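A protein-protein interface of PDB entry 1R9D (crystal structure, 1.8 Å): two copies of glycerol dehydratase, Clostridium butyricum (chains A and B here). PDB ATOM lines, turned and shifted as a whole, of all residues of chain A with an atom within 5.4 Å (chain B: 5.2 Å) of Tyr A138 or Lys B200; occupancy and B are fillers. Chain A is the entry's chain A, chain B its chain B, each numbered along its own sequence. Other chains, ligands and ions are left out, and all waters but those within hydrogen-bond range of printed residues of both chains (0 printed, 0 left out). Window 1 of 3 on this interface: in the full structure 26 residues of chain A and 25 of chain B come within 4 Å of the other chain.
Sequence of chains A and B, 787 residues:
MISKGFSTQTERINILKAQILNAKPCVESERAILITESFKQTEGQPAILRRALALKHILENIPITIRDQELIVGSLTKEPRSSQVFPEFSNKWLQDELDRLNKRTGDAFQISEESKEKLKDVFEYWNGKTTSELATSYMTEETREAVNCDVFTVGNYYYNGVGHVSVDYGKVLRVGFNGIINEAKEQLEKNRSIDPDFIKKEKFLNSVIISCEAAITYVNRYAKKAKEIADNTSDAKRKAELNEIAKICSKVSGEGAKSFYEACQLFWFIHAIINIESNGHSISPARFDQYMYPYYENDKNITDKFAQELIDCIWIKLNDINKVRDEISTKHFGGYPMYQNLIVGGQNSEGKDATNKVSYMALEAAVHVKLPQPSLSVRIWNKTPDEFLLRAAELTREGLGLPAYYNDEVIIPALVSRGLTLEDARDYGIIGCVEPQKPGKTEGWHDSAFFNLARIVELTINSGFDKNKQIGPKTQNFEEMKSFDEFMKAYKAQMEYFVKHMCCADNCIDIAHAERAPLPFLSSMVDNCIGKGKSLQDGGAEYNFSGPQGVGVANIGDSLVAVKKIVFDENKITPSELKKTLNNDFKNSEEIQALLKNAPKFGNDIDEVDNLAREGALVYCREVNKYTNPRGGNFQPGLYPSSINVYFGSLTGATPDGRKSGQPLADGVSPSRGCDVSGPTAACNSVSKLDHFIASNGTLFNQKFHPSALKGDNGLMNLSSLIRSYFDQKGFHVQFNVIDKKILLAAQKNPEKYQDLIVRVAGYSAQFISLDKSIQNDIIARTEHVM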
ATOM      1  N   LEU A 134     -12.048 -17.564   0.464  1.00  0.00           N
ATOM      2  CA  LEU A 134     -13.211 -18.151   1.129  1.00  0.00           C
ATOM      3  C   LEU A 134     -12.866 -19.568   1.609  1.00  0.00           C
ATOM      4  O   LEU A 134     -13.276 -19.979   2.692  1.00  0.00           O
ATOM      5  CB  LEU A 134     -14.402 -18.198   0.170  1.00  0.00           C
ATOM      6  CG  LEU A 134     -15.680 -18.851   0.708  1.00  0.00           C
ATOM      7  CD1 LEU A 134     -16.176 -18.096   1.929  1.00  0.00           C
ATOM      8  CD2 LEU A 134     -16.737 -18.860  -0.383  1.00  0.00           C
ATOM      9  N   ALA A 135     -12.103 -20.304   0.802  1.00  0.00           N
ATOM     10  CA  ALA A 135     -11.705 -21.669   1.158  1.00  0.00           C
ATOM     11  C   ALA A 135     -10.970 -21.676   2.492  1.00  0.00           C
ATOM     12  O   ALA A 135     -11.238 -22.514   3.355  1.00  0.00           O
ATOM     13  CB  ALA A 135     -10.814 -22.262   0.070  1.00  0.00           C
ATOM     14  N   THR A 136     -10.037 -20.742   2.661  1.00  0.00           N
ATOM     15  CA  THR A 136      -9.286 -20.651   3.909  1.00  0.00           C
ATOM     16  C   THR A 136     -10.206 -20.326   5.086  1.00  0.00           C
ATOM     17  O   THR A 136     -10.041 -20.863   6.187  1.00  0.00           O
ATOM     18  CB  THR A 136      -8.177 -19.576   3.807  1.00  0.00           C
ATOM     19  OG1 THR A 136      -7.161 -20.035   2.907  1.00  0.00           O
ATOM     20  CG2 THR A 136      -7.554 -19.307   5.168  1.00  0.00           C
ATOM     21  N   SER A 137     -11.185 -19.456   4.860  1.00  0.00           N
ATOM     22  CA  SER A 137     -12.116 -19.092   5.920  1.00  0.00           C
ATOM     23  C   SER A 137     -12.938 -20.290   6.395  1.00  0.00           C
ATOM     24  O   SER A 137     -13.328 -20.352   7.560  1.00  0.00           O
ATOM     25  CB  SER A 137     -13.058 -17.982   5.445  1.00  0.00           C
ATOM     26  OG  SER A 137     -12.336 -16.797   5.151  1.00  0.00           O
ATOM     27  N   TYR A 138     -13.208 -21.235   5.496  1.00  0.00           N
ATOM     28  CA  TYR A 138     -13.985 -22.421   5.860  1.00  0.00           C
ATOM     29  C   TYR A 138     -13.161 -23.461   6.625  1.00  0.00           C
ATOM     30  O   TYR A 138     -13.716 -24.287   7.348  1.00  0.00           O
ATOM     31  CB  TYR A 138     -14.595 -23.071   4.613  1.00  0.00           C
ATOM     32  CG  TYR A 138     -15.963 -22.536   4.243  1.00  0.00           C
ATOM     33  CD1 TYR A 138     -16.195 -21.959   2.994  1.00  0.00           C
ATOM     34  CD2 TYR A 138     -17.025 -22.607   5.143  1.00  0.00           C
ATOM     35  CE1 TYR A 138     -17.456 -21.462   2.654  1.00  0.00           C
ATOM     36  CE2 TYR A 138     -18.286 -22.114   4.812  1.00  0.00           C
ATOM     37  CZ  TYR A 138     -18.492 -21.543   3.568  1.00  0.00           C
ATOM     38  OH  TYR A 138     -19.732 -21.037   3.248  1.00  0.00           O
ATOM     39  N   MET A 139     -11.840 -23.407   6.477  1.00  0.00           N
ATOM     40  CA  MET A 139     -10.954 -24.351   7.157  1.00  0.00           C
ATOM     41  C   MET A 139     -10.797 -24.022   8.635  1.00  0.00           C
ATOM     42  O   MET A 139     -10.760 -22.854   9.016  1.00  0.00           O
ATOM     43  CB  MET A 139      -9.565 -24.347   6.511  1.00  0.00           C
ATOM     44  CG  MET A 139      -9.515 -24.870   5.099  1.00  0.00           C
ATOM     45  SD  MET A 139      -7.834 -24.814   4.440  1.00  0.00           S
ATOM     46  CE  MET A 139      -8.165 -24.697   2.692  1.00  0.00           C
ATOM     47  N   THR A 140     -10.695 -25.056   9.465  1.00  0.00           N
ATOM     48  CA  THR A 140     -10.508 -24.855  10.898  1.00  0.00           C
ATOM     49  C   THR A 140      -9.041 -24.505  11.116  1.00  0.00           C
ATOM     50  O   THR A 140      -8.207 -24.747  10.246  1.00  0.00           O
ATOM     51  CB  THR A 140     -10.817 -26.128  11.686  1.00  0.00           C
ATOM     52  OG1 THR A 140      -9.879 -27.146  11.322  1.00  0.00           O
ATOM     53  CG2 THR A 140     -12.229 -26.614  11.385  1.00  0.00           C
ATOM     54  N   ARG A 144      -5.672 -25.694   8.942  1.00  0.00           N
ATOM     55  CA  ARG A 144      -4.738 -24.740   8.355  1.00  0.00           C
ATOM     56  C   ARG A 144      -3.307 -25.105   8.737  1.00  0.00           C
ATOM     57  O   ARG A 144      -2.395 -25.038   7.911  1.00  0.00           O
ATOM     58  CB  ARG A 144      -5.056 -23.321   8.834  1.00  0.00           C
ATOM     59  CG  ARG A 144      -6.377 -22.778   8.315  1.00  0.00           C
ATOM     60  CD  ARG A 144      -6.792 -21.522   9.066  1.00  0.00           C
ATOM     61  NE  ARG A 144      -8.089 -21.031   8.611  1.00  0.00           N
ATOM     62  CZ  ARG A 144      -8.969 -20.403   9.386  1.00  0.00           C
ATOM     63  NH1 ARG A 144      -8.697 -20.186  10.667  1.00  0.00           N
ATOM     64  NH2 ARG A 144     -10.123 -19.994   8.880  1.00  0.00           N
ATOM     65  N   CYS A 508     -13.313 -27.946   1.801  1.00  0.00           N
ATOM     66  CA  CYS A 508     -13.527 -26.517   2.015  1.00  0.00           C
ATOM     67  C   CYS A 508     -13.330 -25.754   0.705  1.00  0.00           C
ATOM     68  O   CYS A 508     -14.042 -24.788   0.424  1.00  0.00           O
ATOM     69  CB  CYS A 508     -12.569 -25.982   3.086  1.00  0.00           C
ATOM     70  SG  CYS A 508     -12.935 -26.561   4.768  1.00  0.00           S
ATOM     71  N   ILE A 511     -16.409 -26.399  -1.475  1.00  0.00           N
ATOM     72  CA  ILE A 511     -17.510 -25.519  -1.096  1.00  0.00           C
ATOM     73  C   ILE A 511     -17.281 -24.105  -1.631  1.00  0.00           C
ATOM     74  O   ILE A 511     -18.216 -23.459  -2.098  1.00  0.00           O
ATOM     75  CB  ILE A 511     -17.675 -25.468   0.444  1.00  0.00           C
ATOM     76  CG1 ILE A 511     -18.203 -26.814   0.950  1.00  0.00           C
ATOM     77  CG2 ILE A 511     -18.642 -24.353   0.841  1.00  0.00           C
ATOM     78  CD1 ILE A 511     -18.196 -26.954   2.468  1.00  0.00           C
ATOM     79  N   ALA A 512     -16.036 -23.636  -1.582  1.00  0.00           N
ATOM     80  CA  ALA A 512     -15.712 -22.288  -2.055  1.00  0.00           C
ATOM     81  C   ALA A 512     -15.970 -22.099  -3.547  1.00  0.00           C
ATOM     82  O   ALA A 512     -16.506 -21.066  -3.957  1.00  0.00           O
ATOM     83  CB  ALA A 512     -14.256 -21.945  -1.724  1.00  0.00           C
ATOM     84  N   GLU A 515     -19.667 -21.825  -4.112  1.00  0.00           N
ATOM     85  CA  GLU A 515     -20.212 -20.565  -3.618  1.00  0.00           C
ATOM     86  C   GLU A 515     -19.814 -19.349  -4.443  1.00  0.00           C
ATOM     87  O   GLU A 515     -20.625 -18.444  -4.645  1.00  0.00           O
ATOM     88  CB  GLU A 515     -19.785 -20.354  -2.160  1.00  0.00           C
ATOM     89  CG  GLU A 515     -20.495 -19.217  -1.441  1.00  0.00           C
ATOM     90  CD  GLU A 515     -20.241 -19.229   0.063  1.00  0.00           C
ATOM     91  OE1 GLU A 515     -20.144 -20.339   0.640  1.00  0.00           O
ATOM     92  OE2 GLU A 515     -20.154 -18.134   0.671  1.00  0.00           O
ATOM     93  N   PRO B  46     -17.586 -16.251   5.234  1.00  0.00           N
ATOM     94  CA  PRO B  46     -18.935 -16.693   4.854  1.00  0.00           C
ATOM     95  C   PRO B  46     -19.917 -15.679   5.447  1.00  0.00           C
ATOM     96  O   PRO B  46     -19.630 -15.073   6.476  1.00  0.00           O
ATOM     97  CB  PRO B  46     -19.062 -18.056   5.533  1.00  0.00           C
ATOM     98  CG  PRO B  46     -17.654 -18.525   5.646  1.00  0.00           C
ATOM     99  CD  PRO B  46     -16.900 -17.284   6.027  1.00  0.00           C
ATOM    100  N   PRO B 196     -18.789 -33.600   5.357  1.00  0.00           N
ATOM    101  CA  PRO B 196     -18.693 -32.226   4.841  1.00  0.00           C
ATOM    102  C   PRO B 196     -19.841 -31.316   5.277  1.00  0.00           C
ATOM    103  O   PRO B 196     -19.678 -30.098   5.362  1.00  0.00           O
ATOM    104  CB  PRO B 196     -18.681 -32.422   3.325  1.00  0.00           C
ATOM    105  CG  PRO B 196     -18.123 -33.787   3.156  1.00  0.00           C
ATOM    106  CD  PRO B 196     -18.799 -34.564   4.245  1.00  0.00           C
ATOM    107  N   ASP B 197     -21.003 -31.906   5.543  1.00  0.00           N
ATOM    108  CA  ASP B 197     -22.156 -31.113   5.953  1.00  0.00           C
ATOM    109  C   ASP B 197     -21.955 -30.390   7.276  1.00  0.00           C
ATOM    110  O   ASP B 197     -22.674 -29.440   7.578  1.00  0.00           O
ATOM    111  CB  ASP B 197     -23.415 -31.985   6.036  1.00  0.00           C
ATOM    112  CG  ASP B 197     -23.950 -32.366   4.666  1.00  0.00           C
ATOM    113  OD1 ASP B 197     -23.872 -31.523   3.744  1.00  0.00           O
ATOM    114  OD2 ASP B 197     -24.461 -33.500   4.511  1.00  0.00           O
ATOM    115  N   PHE B 198     -20.984 -30.825   8.070  1.00  0.00           N
ATOM    116  CA  PHE B 198     -20.752 -30.168   9.345  1.00  0.00           C
ATOM    117  C   PHE B 198     -19.874 -28.921   9.238  1.00  0.00           C
ATOM    118  O   PHE B 198     -19.788 -28.140  10.186  1.00  0.00           O
ATOM    119  CB  PHE B 198     -20.178 -31.160  10.362  1.00  0.00           C
ATOM    120  CG  PHE B 198     -21.180 -32.183  10.833  1.00  0.00           C
ATOM    121  CD1 PHE B 198     -21.132 -33.494  10.370  1.00  0.00           C
ATOM    122  CD2 PHE B 198     -22.199 -31.821  11.713  1.00  0.00           C
ATOM    123  CE1 PHE B 198     -22.086 -34.430  10.773  1.00  0.00           C
ATOM    124  CE2 PHE B 198     -23.156 -32.749  12.122  1.00  0.00           C
ATOM    125  CZ  PHE B 198     -23.100 -34.056  11.651  1.00  0.00           C
ATOM    126  N   ILE B 199     -19.246 -28.720   8.083  1.00  0.00           N
ATOM    127  CA  ILE B 199     -18.397 -27.548   7.875  1.00  0.00           C
ATOM    128  C   ILE B 199     -19.223 -26.264   8.011  1.00  0.00           C
ATOM    129  O   ILE B 199     -18.869 -25.368   8.776  1.00  0.00           O
ATOM    130  CB  ILE B 199     -17.724 -27.585   6.483  1.00  0.00           C
ATOM    131  CG1 ILE B 199     -16.729 -28.750   6.422  1.00  0.00           C
ATOM    132  CG2 ILE B 199     -17.007 -26.258   6.209  1.00  0.00           C
ATOM    133  CD1 ILE B 199     -16.147 -29.002   5.054  1.00  0.00           C
ATOM    134  N   LYS B 200     -20.329 -26.172   7.284  1.00  0.00           N
ATOM    135  CA  LYS B 200     -21.159 -24.977   7.385  1.00  0.00           C
ATOM    136  C   LYS B 200     -21.831 -24.865   8.756  1.00  0.00           C
ATOM    137  O   LYS B 200     -22.021 -23.764   9.264  1.00  0.00           O
ATOM    138  CB  LYS B 200     -22.202 -24.951   6.265  1.00  0.00           C
ATOM    139  CG  LYS B 200     -21.615 -24.578   4.906  1.00  0.00           C
ATOM    140  CD  LYS B 200     -22.686 -24.513   3.823  1.00  0.00           C
ATOM    141  CE  LYS B 200     -22.087 -24.135   2.474  1.00  0.00           C
ATOM    142  NZ  LYS B 200     -23.126 -24.015   1.408  1.00  0.00           N
ATOM    143  N   LYS B 201     -22.177 -25.998   9.365  1.00  0.00           N
ATOM    144  CA  LYS B 201     -22.807 -25.965  10.683  1.00  0.00           C
ATOM    145  C   LYS B 201     -21.820 -25.431  11.713  1.00  0.00           C
ATOM    146  O   LYS B 201     -22.190 -24.701  12.630  1.00  0.00           O
ATOM    147  CB  LYS B 201     -23.272 -27.361  11.103  1.00  0.00           C
ATOM    148  CG  LYS B 201     -24.347 -27.963  10.204  1.00  0.00           C
ATOM    149  CD  LYS B 201     -24.892 -29.255  10.797  1.00  0.00           C
ATOM    150  CE  LYS B 201     -25.592 -30.099   9.749  1.00  0.00           C
ATOM    151  NZ  LYS B 201     -26.614 -29.332   8.991  1.00  0.00           N
ATOM    152  N   GLU B 202     -20.556 -25.801  11.549  1.00  0.00           N
ATOM    153  CA  GLU B 202     -19.506 -25.365  12.458  1.00  0.00           C
ATOM    154  C   GLU B 202     -19.373 -23.845  12.412  1.00  0.00           C
ATOM    155  O   GLU B 202     -19.205 -23.197  13.444  1.00  0.00           O
ATOM    156  CB  GLU B 202     -18.190 -26.053  12.073  1.00  0.00           C
ATOM    157  CG  GLU B 202     -16.981 -25.688  12.914  1.00  0.00           C
ATOM    158  CD  GLU B 202     -16.249 -24.479  12.376  1.00  0.00           C
ATOM    159  OE1 GLU B 202     -16.641 -23.341  12.709  1.00  0.00           O
ATOM    160  OE2 GLU B 202     -15.285 -24.670  11.602  1.00  0.00           O
ATOM    161  N   LYS B 203     -19.451 -23.275  11.214  1.00  0.00           N
ATOM    162  CA  LYS B 203     -19.359 -21.828  11.074  1.00  0.00           C
ATOM    163  C   LYS B 203     -20.562 -21.164  11.735  1.00  0.00           C
ATOM    164  O   LYS B 203     -20.428 -20.116  12.358  1.00  0.00           O
ATOM    165  CB  LYS B 203     -19.279 -21.428   9.597  1.00  0.00           C
ATOM    166  CG  LYS B 203     -18.043 -21.963   8.893  1.00  0.00           C
ATOM    167  CD  LYS B 203     -16.777 -21.691   9.709  1.00  0.00           C
ATOM    168  CE  LYS B 203     -15.557 -22.350   9.082  1.00  0.00           C
ATOM    169  NZ  LYS B 203     -14.339 -22.222   9.939  1.00  0.00           N
ATOM    170  N   PHE B 204     -21.736 -21.775  11.609  1.00  0.00           N
ATOM    171  CA  PHE B 204     -22.929 -21.202  12.226  1.00  0.00           C
ATOM    172  C   PHE B 204     -22.802 -21.196  13.746  1.00  0.00           C
ATOM    173  O   PHE B 204     -23.074 -20.187  14.395  1.00  0.00           O
ATOM    174  CB  PHE B 204     -24.190 -21.989  11.853  1.00  0.00           C
ATOM    175  CG  PHE B 204     -25.402 -21.574  12.637  1.00  0.00           C
ATOM    176  CD1 PHE B 204     -26.028 -20.360  12.381  1.00  0.00           C
ATOM    177  CD2 PHE B 204     -25.873 -22.360  13.688  1.00  0.00           C
ATOM    178  CE1 PHE B 204     -27.098 -19.929  13.162  1.00  0.00           C
ATOM    179  CE2 PHE B 204     -26.947 -21.935  14.477  1.00  0.00           C
ATOM    180  CZ  PHE B 204     -27.559 -20.714  14.212  1.00  0.00           C
ATOM    181  N   GLY B 533     -27.937 -26.657  13.715  1.00  0.00           N
ATOM    182  CA  GLY B 533     -26.751 -25.990  13.212  1.00  0.00           C
ATOM    183  C   GLY B 533     -27.079 -25.099  12.029  1.00  0.00           C
ATOM    184  O   GLY B 533     -26.245 -24.910  11.143  1.00  0.00           O
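Among the printed residues, merely in contact across the chains: Thr A140 with Glu B202 (3.6 Å), Tyr A138 with Pro B46 (3.7 Å), Met A139 with Lys B203 (3.7 Å), Tyr A138 with Ile B199 (3.8 Å), Ile A511 with Lys B200 (3.8 Å), Ile A511 with Ile B199 (3.9 Å), Ser A137 with Pro B46 (3.9 Å) and Tyr A138 with Lys B200 (3.97 Å).
Of the printed residues of chain B, Ile A511 touches Ile B199 and Lys B200.
Of the printed residues of chain A, Pro B46 touches Ser A137 (3.9 Å) and Tyr A138 (3.7 Å).
Asp B197 touches none of the printed residues of chain A.
Lys B200 touches just these residues of chain A: Tyr A138 (3.97 Å) and Ile A511 (3.8 Å).
Printed residues of chain A within 4 Å of Glu B202: Thr A140 (3.6 Å).
Of the printed residues of chain A, Lys B203 touches Ser A137, Tyr A138 and Met A139.
Gly B533 touches none of the printed residues of chain A.
The nearest printed residue of chain A that does not touch Glu B202 is Tyr A138 (4.6 Å).
The backbone carbonyl oxygen of Met A139 is in hydrogen-bond range of the guanidinium group of Arg A144.
SG of Cys A508 sits at hydrogen-bond distance from N of Met A139 (3.8 Å).
The backbone carbonyl oxygen (O) of Tyr A138 is in hydrogen-bond range of the side-chain sulfur (SG) of Cys A508.
The side-chain carboxylate (OE2) of Glu B202 lies within salt-bridge range of the side-chain amino group (NZ) of Lys B203 (3.1 Å).
The side-chain hydroxyl of Tyr A138 sits at hydrogen-bond distance from the side-chain carboxylate of Glu A515 (2.7 Å).
O of Ser A137 sits at hydrogen-bond distance from NH2 of Arg A144, at 3.5 Å.
No position is printed for both chains.
Of the 11 printed residues of chain B, 5 touch a printed residue of chain A.
Printed residues of chain B that touch a printed residue of chain A: Pro B46, Ile B199, Lys B200, Glu B202 and Lys B203.
Hydrophobic or aromatic side chains of chain B within 4 Å of the printed part of chain A: Pro B46 and Ile B199.
Along chain B the printed residues that touch a printed residue of chain A span positions 46 to 203.
Hydrophobic or aromatic side chains of chain A within 4 Å of the printed part of chain B: Tyr A138 and Ile A511.
Along chain A the printed residues that touch a printed residue of chain B span positions 137 to 511.
Among the printed residues, 10 pairs touch across the chains.
The backbone carbonyl oxygen (O) of Tyr A138 sits close to the side-chain amino group (NZ) of Lys B203 (3.4 Å).
O of Ser A137 lies within hydrogen-bond range of NZ of Lys B203 (3.2 Å).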
